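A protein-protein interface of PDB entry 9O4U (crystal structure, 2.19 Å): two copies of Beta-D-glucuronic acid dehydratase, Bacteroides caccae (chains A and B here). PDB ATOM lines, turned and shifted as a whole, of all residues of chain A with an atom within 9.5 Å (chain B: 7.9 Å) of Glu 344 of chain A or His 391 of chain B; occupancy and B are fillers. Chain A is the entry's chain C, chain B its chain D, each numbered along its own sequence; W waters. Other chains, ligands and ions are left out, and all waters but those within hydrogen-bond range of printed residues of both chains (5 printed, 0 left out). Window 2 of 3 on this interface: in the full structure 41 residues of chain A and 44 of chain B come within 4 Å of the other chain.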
ATOM      1  N   GLU A  53     -19.825  12.111  20.683  1.00  0.00           N
ATOM      2  CA  GLU A  53     -19.874  13.548  20.469  1.00  0.00           C
ATOM      3  C   GLU A  53     -21.015  14.165  21.270  1.00  0.00           C
ATOM      4  O   GLU A  53     -22.128  13.627  21.303  1.00  0.00           O
ATOM      5  CB  GLU A  53     -20.053  13.849  18.982  1.00  0.00           C
ATOM      6  CG  GLU A  53     -19.906  15.306  18.626  1.00  0.00           C
ATOM      7  CD  GLU A  53     -20.513  15.638  17.282  1.00  0.00           C
ATOM      8  OE1 GLU A  53     -20.860  14.715  16.524  1.00  0.00           O
ATOM      9  OE2 GLU A  53     -20.669  16.835  16.991  1.00  0.00           O
ATOM     10  N   THR A  54     -20.727  15.288  21.939  1.00  0.00           N
ATOM     11  CA  THR A  54     -21.739  16.059  22.656  1.00  0.00           C
ATOM     12  C   THR A  54     -21.506  17.538  22.379  1.00  0.00           C
ATOM     13  O   THR A  54     -20.424  17.942  21.949  1.00  0.00           O
ATOM     14  CB  THR A  54     -21.718  15.809  24.184  1.00  0.00           C
ATOM     15  OG1 THR A  54     -20.489  16.293  24.744  1.00  0.00           O
ATOM     16  CG2 THR A  54     -21.895  14.320  24.514  1.00  0.00           C
ATOM     17  N   ARG A  55     -22.531  18.356  22.628  1.00  0.00           N
ATOM     18  CA  ARG A  55     -22.374  19.782  22.374  1.00  0.00           C
ATOM     19  C   ARG A  55     -21.354  20.407  23.320  1.00  0.00           C
ATOM     20  O   ARG A  55     -20.614  21.317  22.927  1.00  0.00           O
ATOM     21  CB  ARG A  55     -23.710  20.507  22.492  1.00  0.00           C
ATOM     22  CG  ARG A  55     -23.612  21.974  22.074  1.00  0.00           C
ATOM     23  CD  ARG A  55     -24.902  22.741  22.326  1.00  0.00           C
ATOM     24  NE  ARG A  55     -24.758  24.135  21.936  1.00  0.00           N
ATOM     25  CZ  ARG A  55     -25.628  25.094  22.212  1.00  0.00           C
ATOM     26  NH1 ARG A  55     -26.752  24.847  22.871  1.00  0.00           N
ATOM     27  NH2 ARG A  55     -25.363  26.335  21.816  1.00  0.00           N
ATOM     28  N   SER A  56     -21.296  19.928  24.563  1.00  0.00           N
ATOM     29  CA  SER A  56     -20.383  20.482  25.554  1.00  0.00           C
ATOM     30  C   SER A  56     -18.987  19.880  25.475  1.00  0.00           C
ATOM     31  O   SER A  56     -18.048  20.455  26.033  1.00  0.00           O
ATOM     32  CB  SER A  56     -20.938  20.265  26.964  1.00  0.00           C
ATOM     33  OG  SER A  56     -20.925  18.888  27.315  1.00  0.00           O
ATOM     34  N   ALA A 277     -37.135  22.685   9.942  1.00  0.00           N
ATOM     35  CA  ALA A 277     -36.474  22.395  11.211  1.00  0.00           C
ATOM     36  C   ALA A 277     -37.167  23.176  12.322  1.00  0.00           C
ATOM     37  O   ALA A 277     -37.131  24.411  12.334  1.00  0.00           O
ATOM     38  CB  ALA A 277     -34.989  22.757  11.156  1.00  0.00           C
ATOM     39  N   VAL A 282     -34.158  18.306  17.211  1.00  0.00           N
ATOM     40  CA  VAL A 282     -34.197  18.371  15.755  1.00  0.00           C
ATOM     41  C   VAL A 282     -33.104  17.512  15.117  1.00  0.00           C
ATOM     42  O   VAL A 282     -33.208  17.143  13.935  1.00  0.00           O
ATOM     43  CB  VAL A 282     -34.093  19.837  15.301  1.00  0.00           C
ATOM     44  CG1 VAL A 282     -32.634  20.302  15.279  1.00  0.00           C
ATOM     45  CG2 VAL A 282     -34.750  20.019  13.962  1.00  0.00           C
ATOM     46  N   THR A 283     -32.060  17.179  15.882  1.00  0.00           N
ATOM     47  CA  THR A 283     -30.963  16.316  15.463  1.00  0.00           C
ATOM     48  C   THR A 283     -31.398  14.885  15.173  1.00  0.00           C
ATOM     49  O   THR A 283     -30.568  14.087  14.731  1.00  0.00           O
ATOM     50  CB  THR A 283     -29.910  16.293  16.557  1.00  0.00           C
ATOM     51  OG1 THR A 283     -30.546  15.919  17.791  1.00  0.00           O
ATOM     52  CG2 THR A 283     -29.276  17.658  16.710  1.00  0.00           C
ATOM     53  N   VAL A 335     -23.094  12.735  12.889  1.00  0.00           N
ATOM     54  CA  VAL A 335     -22.604  13.837  13.719  1.00  0.00           C
ATOM     55  C   VAL A 335     -23.782  14.687  14.181  1.00  0.00           C
ATOM     56  O   VAL A 335     -24.864  14.682  13.584  1.00  0.00           O
ATOM     57  CB  VAL A 335     -21.570  14.723  12.984  1.00  0.00           C
ATOM     58  CG1 VAL A 335     -20.403  13.889  12.487  1.00  0.00           C
ATOM     59  CG2 VAL A 335     -22.228  15.473  11.838  1.00  0.00           C
ATOM     60  N   LEU A 336     -23.544  15.459  15.244  1.00  0.00           N
ATOM     61  CA  LEU A 336     -24.574  16.327  15.793  1.00  0.00           C
ATOM     62  C   LEU A 336     -24.948  17.403  14.790  1.00  0.00           C
ATOM     63  O   LEU A 336     -24.081  18.124  14.290  1.00  0.00           O
ATOM     64  CB  LEU A 336     -24.087  16.979  17.084  1.00  0.00           C
ATOM     65  CG  LEU A 336     -23.765  16.064  18.260  1.00  0.00           C
ATOM     66  CD1 LEU A 336     -23.134  16.871  19.387  1.00  0.00           C
ATOM     67  CD2 LEU A 336     -25.032  15.342  18.730  1.00  0.00           C
ATOM     68  N   GLY A 337     -26.242  17.514  14.498  1.00  0.00           N
ATOM     69  CA  GLY A 337     -26.728  18.572  13.641  1.00  0.00           C
ATOM     70  C   GLY A 337     -28.003  18.166  12.925  1.00  0.00           C
ATOM     71  O   GLY A 337     -28.683  17.217  13.307  1.00  0.00           O
ATOM     72  N   PHE A 338     -28.307  18.930  11.876  1.00  0.00           N
ATOM     73  CA  PHE A 338     -29.532  18.760  11.098  1.00  0.00           C
ATOM     74  C   PHE A 338     -29.182  18.404   9.658  1.00  0.00           C
ATOM     75  O   PHE A 338     -29.378  17.255   9.245  1.00  0.00           O
ATOM     76  CB  PHE A 338     -30.354  20.044  11.190  1.00  0.00           C
ATOM     77  CG  PHE A 338     -31.646  20.013  10.430  1.00  0.00           C
ATOM     78  CD1 PHE A 338     -32.750  19.333  10.937  1.00  0.00           C
ATOM     79  CD2 PHE A 338     -31.766  20.687   9.224  1.00  0.00           C
ATOM     80  CE1 PHE A 338     -33.946  19.317  10.252  1.00  0.00           C
ATOM     81  CE2 PHE A 338     -32.965  20.678   8.524  1.00  0.00           C
ATOM     82  CZ  PHE A 338     -34.064  19.990   9.043  1.00  0.00           C
ATOM     83  N   ASN A 339     -28.643  19.345   8.889  1.00  0.00           N
ATOM     84  CA  ASN A 339     -28.063  19.037   7.584  1.00  0.00           C
ATOM     85  C   ASN A 339     -26.690  19.705   7.536  1.00  0.00           C
ATOM     86  O   ASN A 339     -26.550  20.842   7.087  1.00  0.00           O
ATOM     87  CB  ASN A 339     -28.954  19.485   6.439  1.00  0.00           C
ATOM     88  CG  ASN A 339     -28.654  18.727   5.164  1.00  0.00           C
ATOM     89  OD1 ASN A 339     -28.563  17.493   5.177  1.00  0.00           O
ATOM     90  ND2 ASN A 339     -28.467  19.454   4.062  1.00  0.00           N
ATOM     91  N   GLY A 340     -25.677  18.976   7.971  1.00  0.00           N
ATOM     92  CA  GLY A 340     -24.355  19.515   8.203  1.00  0.00           C
ATOM     93  C   GLY A 340     -23.916  19.234   9.624  1.00  0.00           C
ATOM     94  O   GLY A 340     -24.640  18.637  10.424  1.00  0.00           O
ATOM     95  N   HIS A 341     -22.696  19.667   9.932  1.00  0.00           N
ATOM     96  CA  HIS A 341     -22.203  19.539  11.298  1.00  0.00           C
ATOM     97  C   HIS A 341     -22.624  20.792  12.045  1.00  0.00           C
ATOM     98  O   HIS A 341     -21.979  21.838  11.943  1.00  0.00           O
ATOM     99  CB  HIS A 341     -20.698  19.331  11.346  1.00  0.00           C
ATOM    100  CG  HIS A 341     -20.236  18.760  12.650  1.00  0.00           C
ATOM    101  ND1 HIS A 341     -18.905  18.582  12.963  1.00  0.00           N
ATOM    102  CD2 HIS A 341     -20.939  18.326  13.725  1.00  0.00           C
ATOM    103  CE1 HIS A 341     -18.808  18.061  14.175  1.00  0.00           C
ATOM    104  NE2 HIS A 341     -20.027  17.898  14.657  1.00  0.00           N
ATOM    105  N   GLN A 342     -23.722  20.685  12.792  1.00  0.00           N
ATOM    106  CA  GLN A 342     -24.330  21.815  13.489  1.00  0.00           C
ATOM    107  C   GLN A 342     -24.558  21.436  14.942  1.00  0.00           C
ATOM    108  O   GLN A 342     -25.704  21.315  15.389  1.00  0.00           O
ATOM    109  CB  GLN A 342     -25.642  22.223  12.817  1.00  0.00           C
ATOM    110  CG  GLN A 342     -25.462  22.642  11.369  1.00  0.00           C
ATOM    111  CD  GLN A 342     -26.659  22.291  10.506  1.00  0.00           C
ATOM    112  OE1 GLN A 342     -27.220  21.196  10.624  1.00  0.00           O
ATOM    113  NE2 GLN A 342     -27.060  23.220   9.632  1.00  0.00           N
ATOM    114  N   PRO A 343     -23.485  21.257  15.720  1.00  0.00           N
ATOM    115  CA  PRO A 343     -23.668  20.862  17.128  1.00  0.00           C
ATOM    116  C   PRO A 343     -24.418  21.900  17.942  1.00  0.00           C
ATOM    117  O   PRO A 343     -24.891  21.579  19.041  1.00  0.00           O
ATOM    118  CB  PRO A 343     -22.230  20.671  17.635  1.00  0.00           C
ATOM    119  CG  PRO A 343     -21.400  21.530  16.743  1.00  0.00           C
ATOM    120  CD  PRO A 343     -22.066  21.487  15.397  1.00  0.00           C
ATOM    121  N   GLU A 344     -24.568  23.121  17.424  1.00  0.00           N
ATOM    122  CA  GLU A 344     -25.260  24.168  18.164  1.00  0.00           C
ATOM    123  C   GLU A 344     -26.764  23.906  18.307  1.00  0.00           C
ATOM    124  O   GLU A 344     -27.410  24.544  19.145  1.00  0.00           O
ATOM    125  CB  GLU A 344     -25.011  25.528  17.495  1.00  0.00           C
ATOM    126  CG  GLU A 344     -25.676  25.715  16.111  1.00  0.00           C
ATOM    127  CD  GLU A 344     -24.866  25.148  14.939  1.00  0.00           C
ATOM    128  OE1 GLU A 344     -23.882  24.418  15.169  1.00  0.00           O
ATOM    129  OE2 GLU A 344     -25.219  25.439  13.774  1.00  0.00           O
ATOM    130  N   CYS A 345     -27.342  22.989  17.531  1.00  0.00           N
ATOM    131  CA  CYS A 345     -28.760  22.677  17.675  1.00  0.00           C
ATOM    132  C   CYS A 345     -29.015  21.391  18.468  1.00  0.00           C
ATOM    133  O   CYS A 345     -30.175  20.986  18.608  1.00  0.00           O
ATOM    134  CB  CYS A 345     -29.429  22.583  16.301  1.00  0.00           C
ATOM    135  SG  CYS A 345     -28.942  21.128  15.351  1.00  0.00           S
ATOM    136  N   ALA A 346     -27.973  20.742  18.992  1.00  0.00           N
ATOM    137  CA  ALA A 346     -28.160  19.543  19.805  1.00  0.00           C
ATOM    138  C   ALA A 346     -28.507  19.913  21.243  1.00  0.00           C
ATOM    139  O   ALA A 346     -27.913  20.827  21.827  1.00  0.00           O
ATOM    140  CB  ALA A 346     -26.906  18.665  19.785  1.00  0.00           C
ATOM    141  N   ASP A 347     -29.501  19.220  21.798  1.00  0.00           N
ATOM    142  CA  ASP A 347     -29.866  19.406  23.190  1.00  0.00           C
ATOM    143  C   ASP A 347     -28.783  18.824  24.086  1.00  0.00           C
ATOM    144  O   ASP A 347     -27.985  17.971  23.671  1.00  0.00           O
ATOM    145  CB  ASP A 347     -31.204  18.737  23.505  1.00  0.00           C
ATOM    146  CG  ASP A 347     -32.362  19.338  22.725  1.00  0.00           C
ATOM    147  OD1 ASP A 347     -32.797  20.464  23.062  1.00  0.00           O
ATOM    148  OD2 ASP A 347     -32.826  18.688  21.760  1.00  0.00           O
ATOM    149  N   GLY A 348     -28.769  19.294  25.334  1.00  0.00           N
ATOM    150  CA  GLY A 348     -27.808  18.803  26.306  1.00  0.00           C
ATOM    151  C   GLY A 348     -27.932  17.321  26.601  1.00  0.00           C
ATOM    152  O   GLY A 348     -26.991  16.726  27.123  1.00  0.00           O
ATOM    153  N   HIS B 304     -32.857  35.823  18.215  1.00  0.00           N
ATOM    154  CA  HIS B 304     -32.203  34.965  17.232  1.00  0.00           C
ATOM    155  C   HIS B 304     -32.898  34.962  15.871  1.00  0.00           C
ATOM    156  O   HIS B 304     -32.406  34.306  14.948  1.00  0.00           O
ATOM    157  CB  HIS B 304     -32.124  33.538  17.776  1.00  0.00           C
ATOM    158  CG  HIS B 304     -33.401  33.081  18.410  1.00  0.00           C
ATOM    159  ND1 HIS B 304     -33.707  33.332  19.731  1.00  0.00           N
ATOM    160  CD2 HIS B 304     -34.469  32.426  17.896  1.00  0.00           C
ATOM    161  CE1 HIS B 304     -34.898  32.828  20.010  1.00  0.00           C
ATOM    162  NE2 HIS B 304     -35.383  32.278  18.912  1.00  0.00           N
ATOM    163  N   ASP B 380     -30.253  34.952   5.141  1.00  0.00           N
ATOM    164  CA  ASP B 380     -30.957  33.689   4.970  1.00  0.00           C
ATOM    165  C   ASP B 380     -31.849  33.416   6.181  1.00  0.00           C
ATOM    166  O   ASP B 380     -31.490  33.725   7.321  1.00  0.00           O
ATOM    167  CB  ASP B 380     -29.959  32.539   4.781  1.00  0.00           C
ATOM    168  CG  ASP B 380     -29.250  32.574   3.424  1.00  0.00           C
ATOM    169  OD1 ASP B 380     -29.878  32.912   2.405  1.00  0.00           O
ATOM    170  OD2 ASP B 380     -28.054  32.236   3.371  1.00  0.00           O
ATOM    171  N   TRP B 381     -33.024  32.848   5.929  1.00  0.00           N
ATOM    172  CA  TRP B 381     -33.920  32.484   7.013  1.00  0.00           C
ATOM    173  C   TRP B 381     -33.551  31.107   7.559  1.00  0.00           C
ATOM    174  O   TRP B 381     -32.639  30.429   7.068  1.00  0.00           O
ATOM    175  CB  TRP B 381     -35.379  32.542   6.557  1.00  0.00           C
ATOM    176  CG  TRP B 381     -35.677  31.882   5.242  1.00  0.00           C
ATOM    177  CD1 TRP B 381     -36.231  30.647   5.047  1.00  0.00           C
ATOM    178  CD2 TRP B 381     -35.453  32.431   3.939  1.00  0.00           C
ATOM    179  NE1 TRP B 381     -36.358  30.391   3.700  1.00  0.00           N
ATOM    180  CE2 TRP B 381     -35.888  31.471   3.000  1.00  0.00           C
ATOM    181  CE3 TRP B 381     -34.926  33.638   3.473  1.00  0.00           C
ATOM    182  CZ2 TRP B 381     -35.821  31.686   1.629  1.00  0.00           C
ATOM    183  CZ3 TRP B 381     -34.849  33.848   2.095  1.00  0.00           C
ATOM    184  CH2 TRP B 381     -35.294  32.878   1.196  1.00  0.00           C
ATOM    185  N   THR B 382     -34.294  30.688   8.587  1.00  0.00           N
ATOM    186  CA  THR B 382     -33.872  29.581   9.437  1.00  0.00           C
ATOM    187  C   THR B 382     -33.644  28.301   8.638  1.00  0.00           C
ATOM    188  O   THR B 382     -32.562  27.707   8.698  1.00  0.00           O
ATOM    189  CB  THR B 382     -34.908  29.348  10.536  1.00  0.00           C
ATOM    190  OG1 THR B 382     -34.975  30.506  11.384  1.00  0.00           O
ATOM    191  CG2 THR B 382     -34.535  28.122  11.350  1.00  0.00           C
ATOM    192  N   SER B 383     -34.658  27.848   7.898  1.00  0.00           N
ATOM    193  CA  SER B 383     -34.507  26.586   7.176  1.00  0.00           C
ATOM    194  C   SER B 383     -33.481  26.706   6.060  1.00  0.00           C
ATOM    195  O   SER B 383     -32.785  25.733   5.752  1.00  0.00           O
ATOM    196  CB  SER B 383     -35.848  26.123   6.602  1.00  0.00           C
ATOM    197  OG  SER B 383     -36.097  26.761   5.361  1.00  0.00           O
ATOM    198  N   LYS B 384     -33.367  27.890   5.456  1.00  0.00           N
ATOM    199  CA  LYS B 384     -32.375  28.088   4.406  1.00  0.00           C
ATOM    200  C   LYS B 384     -30.956  27.950   4.954  1.00  0.00           C
ATOM    201  O   LYS B 384     -30.090  27.363   4.299  1.00  0.00           O
ATOM    202  CB  LYS B 384     -32.575  29.450   3.754  1.00  0.00           C
ATOM    203  CG  LYS B 384     -31.781  29.641   2.474  1.00  0.00           C
ATOM    204  CD  LYS B 384     -32.304  30.842   1.709  1.00  0.00           C
ATOM    205  CE  LYS B 384     -31.562  31.043   0.386  1.00  0.00           C
ATOM    206  NZ  LYS B 384     -32.177  32.167  -0.381  1.00  0.00           N
ATOM    207  N   LYS B 385     -30.713  28.473   6.159  1.00  0.00           N
ATOM    208  CA  LYS B 385     -29.444  28.250   6.846  1.00  0.00           C
ATOM    209  C   LYS B 385     -29.279  26.786   7.246  1.00  0.00           C
ATOM    210  O   LYS B 385     -28.218  26.184   7.030  1.00  0.00           O
ATOM    211  CB  LYS B 385     -29.358  29.145   8.088  1.00  0.00           C
ATOM    212  CG  LYS B 385     -28.719  30.500   7.858  1.00  0.00           C
ATOM    213  CD  LYS B 385     -28.400  31.192   9.184  1.00  0.00           C
ATOM    214  CE  LYS B 385     -29.666  31.505   9.978  1.00  0.00           C
ATOM    215  NZ  LYS B 385     -29.351  32.416  11.113  1.00  0.00           N
ATOM    216  N   ALA B 386     -30.319  26.202   7.846  1.00  0.00           N
ATOM    217  CA  ALA B 386     -30.213  24.844   8.363  1.00  0.00           C
ATOM    218  C   ALA B 386     -29.840  23.858   7.265  1.00  0.00           C
ATOM    219  O   ALA B 386     -28.974  22.998   7.462  1.00  0.00           O
ATOM    220  CB  ALA B 386     -31.530  24.436   9.023  1.00  0.00           C
ATOM    221  N   TRP B 387     -30.468  23.977   6.095  1.00  0.00           N
ATOM    222  CA  TRP B 387     -30.279  22.983   5.050  1.00  0.00           C
ATOM    223  C   TRP B 387     -28.971  23.145   4.283  1.00  0.00           C
ATOM    224  O   TRP B 387     -28.595  22.222   3.550  1.00  0.00           O
ATOM    225  CB  TRP B 387     -31.475  23.019   4.100  1.00  0.00           C
ATOM    226  CG  TRP B 387     -32.618  22.219   4.640  1.00  0.00           C
ATOM    227  CD1 TRP B 387     -33.737  22.692   5.280  1.00  0.00           C
ATOM    228  CD2 TRP B 387     -32.734  20.791   4.628  1.00  0.00           C
ATOM    229  NE1 TRP B 387     -34.549  21.639   5.647  1.00  0.00           N
ATOM    230  CE2 TRP B 387     -33.955  20.464   5.257  1.00  0.00           C
ATOM    231  CE3 TRP B 387     -31.929  19.754   4.132  1.00  0.00           C
ATOM    232  CZ2 TRP B 387     -34.384  19.146   5.405  1.00  0.00           C
ATOM    233  CZ3 TRP B 387     -32.349  18.454   4.288  1.00  0.00           C
ATOM    234  CH2 TRP B 387     -33.576  18.159   4.904  1.00  0.00           C
ATOM    235  N   LYS B 388     -28.271  24.275   4.451  1.00  0.00           N
ATOM    236  CA  LYS B 388     -26.954  24.535   3.874  1.00  0.00           C
ATOM    237  C   LYS B 388     -25.815  24.125   4.789  1.00  0.00           C
ATOM    238  O   LYS B 388     -24.658  24.132   4.355  1.00  0.00           O
ATOM    239  CB  LYS B 388     -26.793  26.033   3.563  1.00  0.00           C
ATOM    240  CG  LYS B 388     -27.078  26.424   2.136  1.00  0.00           C
ATOM    241  CD  LYS B 388     -27.856  27.734   2.057  1.00  0.00           C
ATOM    242  CE  LYS B 388     -27.102  28.900   2.686  1.00  0.00           C
ATOM    243  NZ  LYS B 388     -27.124  30.098   1.782  1.00  0.00           N
ATOM    244  N   GLY B 389     -26.108  23.799   6.045  1.00  0.00           N
ATOM    245  CA  GLY B 389     -25.086  23.552   7.035  1.00  0.00           C
ATOM    246  C   GLY B 389     -24.676  24.773   7.816  1.00  0.00           C
ATOM    247  O   GLY B 389     -23.657  24.729   8.514  1.00  0.00           O
ATOM    248  N   GLY B 390     -25.426  25.863   7.709  1.00  0.00           N
ATOM    249  CA  GLY B 390     -25.141  27.063   8.456  1.00  0.00           C
ATOM    250  C   GLY B 390     -25.631  26.950   9.883  1.00  0.00           C
ATOM    251  O   GLY B 390     -26.143  25.921  10.328  1.00  0.00           O
ATOM    252  N   HIS B 391     -25.481  28.058  10.604  1.00  0.00           N
ATOM    253  CA  HIS B 391     -25.867  28.101  12.001  1.00  0.00           C
ATOM    254  C   HIS B 391     -27.357  27.829  12.157  1.00  0.00           C
ATOM    255  O   HIS B 391     -28.189  28.456  11.493  1.00  0.00           O
ATOM    256  CB  HIS B 391     -25.509  29.457  12.598  1.00  0.00           C
ATOM    257  CG  HIS B 391     -25.583  29.487  14.091  1.00  0.00           C
ATOM    258  ND1 HIS B 391     -26.700  29.922  14.771  1.00  0.00           N
ATOM    259  CD2 HIS B 391     -24.687  29.112  15.035  1.00  0.00           C
ATOM    260  CE1 HIS B 391     -26.484  29.824  16.072  1.00  0.00           C
ATOM    261  NE2 HIS B 391     -25.271  29.335  16.258  1.00  0.00           N
ATOM    262  N   LEU B 392     -27.686  26.876  13.032  1.00  0.00           N
ATOM    263  CA  LEU B 392     -29.068  26.545  13.375  1.00  0.00           C
ATOM    264  C   LEU B 392     -29.270  26.760  14.871  1.00  0.00           C
ATOM    265  O   LEU B 392     -28.758  25.994  15.691  1.00  0.00           O
ATOM    266  CB  LEU B 392     -29.410  25.110  12.971  1.00  0.00           C
ATOM    267  CG  LEU B 392     -30.816  24.657  13.354  1.00  0.00           C
ATOM    268  CD1 LEU B 392     -31.837  25.638  12.798  1.00  0.00           C
ATOM    269  CD2 LEU B 392     -31.096  23.246  12.853  1.00  0.00           C
ATOM    270  N   HIS B 393     -30.033  27.788  15.222  1.00  0.00           N
ATOM    271  CA  HIS B 393     -30.377  28.041  16.615  1.00  0.00           C
ATOM    272  C   HIS B 393     -31.278  26.934  17.181  1.00  0.00           C
ATOM    273  O   HIS B 393     -32.205  26.456  16.522  1.00  0.00           O
ATOM    274  CB  HIS B 393     -31.054  29.411  16.735  1.00  0.00           C
ATOM    275  CG  HIS B 393     -31.338  29.829  18.148  1.00  0.00           C
ATOM    276  ND1 HIS B 393     -32.598  29.758  18.709  1.00  0.00           N
ATOM    277  CD2 HIS B 393     -30.525  30.316  19.116  1.00  0.00           C
ATOM    278  CE1 HIS B 393     -32.547  30.186  19.958  1.00  0.00           C
ATOM    279  NE2 HIS B 393     -31.300  30.526  20.232  1.00  0.00           N
ATOM    280  N   LYS B 394     -31.007  26.545  18.424  1.00  0.00           N
ATOM    281  CA  LYS B 394     -31.727  25.451  19.063  1.00  0.00           C
ATOM    282  C   LYS B 394     -33.140  25.878  19.438  1.00  0.00           C
ATOM    283  O   LYS B 394     -33.336  26.886  20.120  1.00  0.00           O
ATOM    284  CB  LYS B 394     -30.984  24.981  20.316  1.00  0.00           C
ATOM    285  CG  LYS B 394     -31.400  23.599  20.765  1.00  0.00           C
ATOM    286  CD  LYS B 394     -30.697  23.154  22.040  1.00  0.00           C
ATOM    287  CE  LYS B 394     -31.080  24.035  23.222  1.00  0.00           C
ATOM    288  NZ  LYS B 394     -30.563  23.477  24.505  1.00  0.00           N
ATOM    289  N   ASP B 395     -34.121  25.086  19.028  1.00  0.00           N
ATOM    290  CA  ASP B 395     -35.505  25.338  19.393  1.00  0.00           C
ATOM    291  C   ASP B 395     -35.927  24.426  20.542  1.00  0.00           C
ATOM    292  O   ASP B 395     -35.364  23.351  20.756  1.00  0.00           O
ATOM    293  CB  ASP B 395     -36.433  25.138  18.190  1.00  0.00           C
ATOM    294  CG  ASP B 395     -37.761  25.841  18.361  1.00  0.00           C
ATOM    295  OD1 ASP B 395     -37.812  26.849  19.099  1.00  0.00           O
ATOM    296  OD2 ASP B 395     -38.757  25.392  17.765  1.00  0.00           O
HETATM  297  O   HOH W   1     -28.586  27.101  19.397  1.00  0.00           O
HETATM  298  O   HOH W   2     -24.975  20.833   4.776  1.00  0.00           O
HETATM  299  O   HOH W   3     -27.931  22.514  24.235  1.00  0.00           O
HETATM  300  O   HOH W   4     -32.180  21.076  25.652  1.00  0.00           O
HETATM  301  O   HOH W   5     -29.828  21.598  27.014  1.00  0.00           O
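Among the printed residues, merely in contact across the chains: Phe 338 of chain A with Ala 386 of chain B, Phe 338 of chain A with Trp 387 of chain B, Phe 338 of chain A with Leu 392 of chain B, Gln 342 of chain A with Gly 389 of chain B, Glu 344 of chain A with Gly 390 of chain B, Glu 344 of chain A with His 391 of chain B, Glu 344 of chain A with Lys 394 of chain B, Cys 345 of chain A with Leu 392 of chain B, Cys 345 of chain A with Lys 394 of chain B, Ala 346 of chain A with Lys 394 of chain B and Asp 347 of chain A with Lys 394 of chain B.
O of Leu 336 of chain A lies within hydrogen-bond range of N of Gln 342 of chain A, at 3.0 Å.
O of Gln 342 of chain A sits at hydrogen-bond distance from SG of Cys 345 of chain A.
The backbone NH (N) of Gly 390 of chain B lies within hydrogen-bond range of the backbone carbonyl oxygen (O) of Lys 385 of chain B, 2.9 Å away.
The side-chain amide oxygen of Gln 342 of chain A sits at hydrogen-bond distance from the backbone NH of Phe 338 of chain A, at 2.8 Å.
Glu 344 of chain A touches four residues of chain B.
Of the printed residues of chain A, His 391 of chain B touches Glu 344.
Gly 390 of chain B touches just these residues of chain A: Gln 342 and Glu 344.
Of the printed residues of chain A, Ala 386 of chain B touches Phe 338, Asn 339 and Gln 342.
Printed residues of chain B within 4 Å of Asp 347 of chain A: Lys 394.
Of the printed residues of chain B, Phe 338 of chain A touches Ala 386 (3.8 Å), Trp 387 (3.4 Å) and Leu 392 (3.7 Å).
Of the printed residues of chain B, Asn 339 of chain A touches Ala 386, Trp 387 and Gly 389.
The nearest residue of chain B that does not touch Glu 344 of chain A is His 393 of chain B (4.9 Å).
The nearest residue of chain A that does not touch His 391 of chain B is Gln 342 of chain A (5.2 Å).
The nearest printed residue of chain B that does not touch Asn 339 of chain A is Lys 388 of chain B (4.1 Å).
No position is printed for both chains.
The backbone NH (N) of Leu 392 of chain B lies within hydrogen-bond range of the side-chain carboxylate (OE2) of Glu 344 of chain A, 2.9 Å away.
The backbone carbonyl oxygen (O) of Asn 339 of chain A sits close to the backbone NH (N) of Gly 389 of chain B, at 3.2 Å.
O of Ala 386 of chain B sits close to O of Asn 339 of chain A (3.3 Å).
The backbone carbonyl oxygen (O) of Trp 387 of chain B lies within hydrogen-bond range of the side-chain amide nitrogen (ND2) of Asn 339 of chain A (2.8 Å).
The side-chain amide nitrogen (NE2) of Gln 342 of chain A is in hydrogen-bond range of the backbone carbonyl oxygen (O) of Ala 386 of chain B, 2.9 Å away.
NE2 of Gln 342 of chain A is in hydrogen-bond range of O of Gly 390 of chain B, 2.9 Å away.
Hydrophobic or aromatic side chains of chain A that line the printed part of chain B: Phe 338.
Of the 17 printed residues of chain B, 7 touch a printed residue of chain A.
Hydrophobic or aromatic side chains of chain B that line the printed part of chain A: Ala 386, Trp 387, His 391 and Leu 392.
Among the printed residues, no Asp or Glu carboxylate lies within 4 Å of a Lys or Arg side-chain nitrogen of the other chain.
Water W2 lies within hydrogen-bond range of the backbone carbonyl oxygen of Asn 339 of chain A (2.8 Å), the backbone carbonyl oxygen of Lys 388 of chain B (3.3 Å) and the backbone NH of Gly 389 of chain B (3.4 Å).
Water W3 lies within hydrogen-bond range of the side-chain amino group of Lys 394 of chain B, the backbone carbonyl oxygen of Ala 346 of chain A and the guanidinium group of Arg 55 of chain A.
Water W5 bridges N of Gly 348 of chain A and NZ of Lys 394 of chain B.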
